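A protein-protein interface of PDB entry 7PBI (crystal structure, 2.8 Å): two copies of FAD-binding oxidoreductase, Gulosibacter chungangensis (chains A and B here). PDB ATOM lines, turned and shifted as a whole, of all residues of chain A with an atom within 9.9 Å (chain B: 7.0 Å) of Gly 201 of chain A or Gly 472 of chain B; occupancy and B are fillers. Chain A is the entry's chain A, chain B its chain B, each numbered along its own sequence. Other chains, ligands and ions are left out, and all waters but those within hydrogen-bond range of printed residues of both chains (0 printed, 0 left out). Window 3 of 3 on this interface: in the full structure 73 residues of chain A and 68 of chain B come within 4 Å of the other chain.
The side-chain hydroxyl of Ser 202 of chain A lies close to the backbone carbonyl oxygen of Gly 472 of chain B, at 3.4 Å.
The backbone NH of Ala 204 of chain A sits at hydrogen-bond distance from the side-chain hydroxyl of Ser 202 of chain A. The backbone NH of Val 401 of chain B sits at hydrogen-bond distance from the backbone carbonyl oxygen of Gly 474 of chain B (2.8 Å).
Met 196 of chain A touches Gly 474 of chain B (CE to O, 3.8 Å). Gly 472 of chain B touches Leu 199 of chain A (CA to CD2, 3.6 Å). CD1 of Leu 199 of chain A touches CA of Gly 474 of chain B, 3.3 Å away. CA of Gly 472 of chain B touches O of Gly 201 of chain A (3.96 Å). Ala 403 of chain B touches Leu 207 of chain A (CA to CD1, 3.6 Å).
Printed residues of chain B within 4 Å of Leu 199 of chain A: Gly 472 (3.6 Å) and Gly 474 (3.3 Å). Of chain B, only Gly 472 comes within 4 Å of Gly 201 of chain A. Of the printed residues of chain B, Ser 202 of chain A touches Gly 472 (3.3 Å). Ser 402 of chain B touches none of the printed residues of chain A. Gly 472 of chain B touches just these residues of chain A: Leu 199 (3.6 Å), Gly 201 (3.96 Å) and Ser 202 (3.3 Å).
Hydrophobic or aromatic side chains of chain A that line the printed part of chain B: Met 196, Leu 199 and Leu 207. Of the 11 printed residues of chain B, 3 touch a printed residue of chain A. Hydrophobic or aromatic side chains of chain B that line the printed part of chain A: Ala 403. Among the printed residues, 6 pairs touch across the chains. Among the printed residues, no Asp or Glu carboxylate lies within 4 Å of a Lys or Arg side-chain nitrogen of the other chain.
No position is printed for both chains. Of the 6 pairs that touch across the chains among the printed residues, none has its exchanged pair printed and touching as well.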
ATOM      1  N   ARG A 193      31.608  15.728  18.667  1.00  0.00           N
ATOM      2  CA  ARG A 193      30.150  15.843  18.873  1.00  0.00           C
ATOM      3  C   ARG A 193      29.551  16.649  17.731  1.00  0.00           C
ATOM      4  O   ARG A 193      29.910  17.838  17.581  1.00  0.00           O
ATOM      5  CB  ARG A 193      29.892  16.524  20.208  1.00  0.00           C
ATOM      6  CG  ARG A 193      30.316  15.657  21.374  1.00  0.00           C
ATOM      7  CD  ARG A 193      29.933  16.257  22.707  1.00  0.00           C
ATOM      8  NE  ARG A 193      30.155  15.229  23.703  1.00  0.00           N
ATOM      9  CZ  ARG A 193      29.554  15.167  24.871  1.00  0.00           C
ATOM     10  NH1 ARG A 193      28.701  16.108  25.228  1.00  0.00           N
ATOM     11  NH2 ARG A 193      29.808  14.155  25.675  1.00  0.00           N
ATOM     12  N   MET A 196      24.824  20.815  17.449  1.00  0.00           N
ATOM     13  CA  MET A 196      24.858  21.761  18.593  1.00  0.00           C
ATOM     14  C   MET A 196      25.568  21.129  19.792  1.00  0.00           C
ATOM     15  O   MET A 196      25.786  21.837  20.788  1.00  0.00           O
ATOM     16  CB  MET A 196      23.446  22.184  18.999  1.00  0.00           C
ATOM     17  CG  MET A 196      22.807  23.096  17.987  1.00  0.00           C
ATOM     18  SD  MET A 196      23.632  24.699  17.888  1.00  0.00           S
ATOM     19  CE  MET A 196      22.812  25.316  16.420  1.00  0.00           C
ATOM     20  N   GLY A 197      25.915  19.850  19.705  1.00  0.00           N
ATOM     21  CA  GLY A 197      26.739  19.167  20.717  1.00  0.00           C
ATOM     22  C   GLY A 197      28.135  19.759  20.767  1.00  0.00           C
ATOM     23  O   GLY A 197      28.782  19.673  21.821  1.00  0.00           O
ATOM     24  N   GLY A 198      28.587  20.353  19.664  1.00  0.00           N
ATOM     25  CA  GLY A 198      29.868  21.071  19.623  1.00  0.00           C
ATOM     26  C   GLY A 198      29.858  22.300  20.515  1.00  0.00           C
ATOM     27  O   GLY A 198      30.936  22.869  20.699  1.00  0.00           O
ATOM     28  N   LEU A 199      28.692  22.718  21.027  1.00  0.00           N
ATOM     29  CA  LEU A 199      28.544  23.945  21.855  1.00  0.00           C
ATOM     30  C   LEU A 199      28.415  23.556  23.322  1.00  0.00           C
ATOM     31  O   LEU A 199      27.444  22.923  23.730  1.00  0.00           O
ATOM     32  CB  LEU A 199      27.342  24.782  21.408  1.00  0.00           C
ATOM     33  CG  LEU A 199      27.399  26.230  21.911  1.00  0.00           C
ATOM     34  CD1 LEU A 199      26.827  27.214  20.911  1.00  0.00           C
ATOM     35  CD2 LEU A 199      26.693  26.394  23.246  1.00  0.00           C
ATOM     36  N   PRO A 200      29.384  23.942  24.172  1.00  0.00           N
ATOM     37  CA  PRO A 200      29.286  23.683  25.601  1.00  0.00           C
ATOM     38  C   PRO A 200      27.977  24.241  26.157  1.00  0.00           C
ATOM     39  O   PRO A 200      27.728  25.405  25.968  1.00  0.00           O
ATOM     40  CB  PRO A 200      30.475  24.439  26.200  1.00  0.00           C
ATOM     41  CG  PRO A 200      31.473  24.498  25.078  1.00  0.00           C
ATOM     42  CD  PRO A 200      30.644  24.602  23.811  1.00  0.00           C
ATOM     43  N   GLY A 201      27.192  23.397  26.815  1.00  0.00           N
ATOM     44  CA  GLY A 201      26.032  23.828  27.609  1.00  0.00           C
ATOM     45  C   GLY A 201      24.756  23.861  26.793  1.00  0.00           C
ATOM     46  O   GLY A 201      23.698  24.118  27.396  1.00  0.00           O
ATOM     47  N   SER A 202      24.823  23.600  25.484  1.00  0.00           N
ATOM     48  CA  SER A 202      23.638  23.651  24.588  1.00  0.00           C
ATOM     49  C   SER A 202      22.732  22.439  24.814  1.00  0.00           C
ATOM     50  O   SER A 202      23.231  21.301  24.784  1.00  0.00           O
ATOM     51  CB  SER A 202      24.012  23.726  23.148  1.00  0.00           C
ATOM     52  OG  SER A 202      22.842  23.616  22.354  1.00  0.00           O
ATOM     53  N   GLU A 203      21.432  22.690  24.929  1.00  0.00           N
ATOM     54  CA  GLU A 203      20.385  21.649  25.064  1.00  0.00           C
ATOM     55  C   GLU A 203      19.754  21.323  23.705  1.00  0.00           C
ATOM     56  O   GLU A 203      18.703  20.671  23.705  1.00  0.00           O
ATOM     57  CB  GLU A 203      19.313  22.135  26.039  1.00  0.00           C
ATOM     58  CG  GLU A 203      19.839  22.299  27.449  1.00  0.00           C
ATOM     59  CD  GLU A 203      19.038  23.252  28.315  1.00  0.00           C
ATOM     60  OE1 GLU A 203      18.150  23.950  27.777  1.00  0.00           O
ATOM     61  OE2 GLU A 203      19.302  23.291  29.529  1.00  0.00           O
ATOM     62  N   ALA A 204      20.349  21.732  22.588  1.00  0.00           N
ATOM     63  CA  ALA A 204      19.770  21.492  21.244  1.00  0.00           C
ATOM     64  C   ALA A 204      20.453  20.322  20.517  1.00  0.00           C
ATOM     65  O   ALA A 204      20.039  20.048  19.386  1.00  0.00           O
ATOM     66  CB  ALA A 204      19.834  22.757  20.427  1.00  0.00           C
ATOM     67  N   TRP A 205      21.412  19.633  21.146  1.00  0.00           N
ATOM     68  CA  TRP A 205      22.219  18.545  20.520  1.00  0.00           C
ATOM     69  C   TRP A 205      21.307  17.564  19.783  1.00  0.00           C
ATOM     70  O   TRP A 205      21.677  17.151  18.685  1.00  0.00           O
ATOM     71  CB  TRP A 205      23.077  17.803  21.556  1.00  0.00           C
ATOM     72  CG  TRP A 205      24.113  16.872  20.992  1.00  0.00           C
ATOM     73  CD1 TRP A 205      24.503  16.722  19.689  1.00  0.00           C
ATOM     74  CD2 TRP A 205      24.954  15.983  21.753  1.00  0.00           C
ATOM     75  NE1 TRP A 205      25.504  15.793  19.584  1.00  0.00           N
ATOM     76  CE2 TRP A 205      25.799  15.322  20.834  1.00  0.00           C
ATOM     77  CE3 TRP A 205      25.056  15.674  23.115  1.00  0.00           C
ATOM     78  CZ2 TRP A 205      26.732  14.374  21.243  1.00  0.00           C
ATOM     79  CZ3 TRP A 205      25.974  14.736  23.515  1.00  0.00           C
ATOM     80  CH2 TRP A 205      26.802  14.103  22.590  1.00  0.00           C
ATOM     81  N   LEU A 207      18.013  18.172  19.097  1.00  0.00           N
ATOM     82  CA  LEU A 207      16.848  18.995  18.675  1.00  0.00           C
ATOM     83  C   LEU A 207      17.037  19.500  17.243  1.00  0.00           C
ATOM     84  O   LEU A 207      16.101  19.305  16.450  1.00  0.00           O
ATOM     85  CB  LEU A 207      16.686  20.152  19.663  1.00  0.00           C
ATOM     86  CG  LEU A 207      16.541  19.727  21.124  1.00  0.00           C
ATOM     87  CD1 LEU A 207      16.141  20.900  22.000  1.00  0.00           C
ATOM     88  CD2 LEU A 207      15.523  18.607  21.271  1.00  0.00           C
ATOM     89  N   VAL B 401      19.824  29.328  18.022  1.00  0.00           N
ATOM     90  CA  VAL B 401      18.887  28.175  18.120  1.00  0.00           C
ATOM     91  C   VAL B 401      18.926  27.625  19.547  1.00  0.00           C
ATOM     92  O   VAL B 401      20.026  27.535  20.127  1.00  0.00           O
ATOM     93  CB  VAL B 401      19.244  27.104  17.080  1.00  0.00           C
ATOM     94  CG1 VAL B 401      18.616  25.755  17.393  1.00  0.00           C
ATOM     95  CG2 VAL B 401      18.848  27.587  15.699  1.00  0.00           C
ATOM     96  N   SER B 402      17.761  27.287  20.089  1.00  0.00           N
ATOM     97  CA  SER B 402      17.617  26.847  21.496  1.00  0.00           C
ATOM     98  C   SER B 402      16.482  25.837  21.623  1.00  0.00           C
ATOM     99  O   SER B 402      15.705  25.672  20.670  1.00  0.00           O
ATOM    100  CB  SER B 402      17.409  28.023  22.411  1.00  0.00           C
ATOM    101  OG  SER B 402      16.158  28.650  22.176  1.00  0.00           O
ATOM    102  N   ALA B 403      16.428  25.175  22.775  1.00  0.00           N
ATOM    103  CA  ALA B 403      15.340  24.255  23.167  1.00  0.00           C
ATOM    104  C   ALA B 403      14.067  25.081  23.276  1.00  0.00           C
ATOM    105  O   ALA B 403      14.087  26.121  23.928  1.00  0.00           O
ATOM    106  CB  ALA B 403      15.682  23.579  24.469  1.00  0.00           C
ATOM    107  N   ALA B 467      26.740  36.331  24.948  1.00  0.00           N
ATOM    108  CA  ALA B 467      25.647  36.074  25.911  1.00  0.00           C
ATOM    109  C   ALA B 467      24.890  34.814  25.498  1.00  0.00           C
ATOM    110  O   ALA B 467      24.569  34.022  26.379  1.00  0.00           O
ATOM    111  CB  ALA B 467      24.717  37.256  25.995  1.00  0.00           C
ATOM    112  N   GLY B 468      24.585  34.647  24.213  1.00  0.00           N
ATOM    113  CA  GLY B 468      23.998  33.395  23.704  1.00  0.00           C
ATOM    114  C   GLY B 468      24.900  32.215  24.031  1.00  0.00           C
ATOM    115  O   GLY B 468      24.418  31.221  24.592  1.00  0.00           O
ATOM    116  N   ALA B 469      26.185  32.319  23.714  1.00  0.00           N
ATOM    117  CA  ALA B 469      27.185  31.272  24.006  1.00  0.00           C
ATOM    118  C   ALA B 469      27.203  31.006  25.514  1.00  0.00           C
ATOM    119  O   ALA B 469      27.503  29.875  25.911  1.00  0.00           O
ATOM    120  CB  ALA B 469      28.542  31.705  23.511  1.00  0.00           C
ATOM    121  N   GLU B 470      26.922  32.023  26.328  1.00  0.00           N
ATOM    122  CA  GLU B 470      27.032  31.917  27.804  1.00  0.00           C
ATOM    123  C   GLU B 470      25.894  31.033  28.304  1.00  0.00           C
ATOM    124  O   GLU B 470      26.117  30.324  29.283  1.00  0.00           O
ATOM    125  CB  GLU B 470      27.010  33.297  28.468  1.00  0.00           C
ATOM    126  CG  GLU B 470      28.393  33.864  28.767  1.00  0.00           C
ATOM    127  CD  GLU B 470      29.175  33.193  29.891  1.00  0.00           C
ATOM    128  OE1 GLU B 470      28.550  32.512  30.739  1.00  0.00           O
ATOM    129  OE2 GLU B 470      30.418  33.371  29.927  1.00  0.00           O
ATOM    130  N   GLU B 471      24.742  31.079  27.630  1.00  0.00           N
ATOM    131  CA  GLU B 471      23.482  30.406  28.031  1.00  0.00           C
ATOM    132  C   GLU B 471      23.290  29.128  27.217  1.00  0.00           C
ATOM    133  O   GLU B 471      22.247  28.502  27.386  1.00  0.00           O
ATOM    134  CB  GLU B 471      22.285  31.327  27.788  1.00  0.00           C
ATOM    135  CG  GLU B 471      22.219  32.511  28.730  1.00  0.00           C
ATOM    136  CD  GLU B 471      21.826  32.146  30.150  1.00  0.00           C
ATOM    137  OE1 GLU B 471      20.931  31.287  30.327  1.00  0.00           O
ATOM    138  OE2 GLU B 471      22.431  32.703  31.078  1.00  0.00           O
ATOM    139  N   GLY B 472      24.226  28.790  26.334  1.00  0.00           N
ATOM    140  CA  GLY B 472      24.147  27.570  25.506  1.00  0.00           C
ATOM    141  C   GLY B 472      23.279  27.735  24.266  1.00  0.00           C
ATOM    142  O   GLY B 472      22.690  26.721  23.835  1.00  0.00           O
ATOM    143  N   TYR B 473      23.184  28.948  23.710  1.00  0.00           N
ATOM    144  CA  TYR B 473      22.430  29.245  22.460  1.00  0.00           C
ATOM    145  C   TYR B 473      23.432  29.460  21.322  1.00  0.00           C
ATOM    146  O   TYR B 473      24.229  30.414  21.379  1.00  0.00           O
ATOM    147  CB  TYR B 473      21.518  30.472  22.601  1.00  0.00           C
ATOM    148  CG  TYR B 473      20.633  30.519  23.822  1.00  0.00           C
ATOM    149  CD1 TYR B 473      19.993  29.387  24.299  1.00  0.00           C
ATOM    150  CD2 TYR B 473      20.411  31.716  24.488  1.00  0.00           C
ATOM    151  CE1 TYR B 473      19.175  29.434  25.418  1.00  0.00           C
ATOM    152  CE2 TYR B 473      19.588  31.783  25.604  1.00  0.00           C
ATOM    153  CZ  TYR B 473      18.962  30.637  26.074  1.00  0.00           C
ATOM    154  OH  TYR B 473      18.146  30.685  27.171  1.00  0.00           O
ATOM    155  N   GLY B 474      23.374  28.596  20.310  1.00  0.00           N
ATOM    156  CA  GLY B 474      24.324  28.570  19.186  1.00  0.00           C
ATOM    157  C   GLY B 474      23.715  29.176  17.939  1.00  0.00           C
ATOM    158  O   GLY B 474      22.549  28.866  17.641  1.00  0.00           O
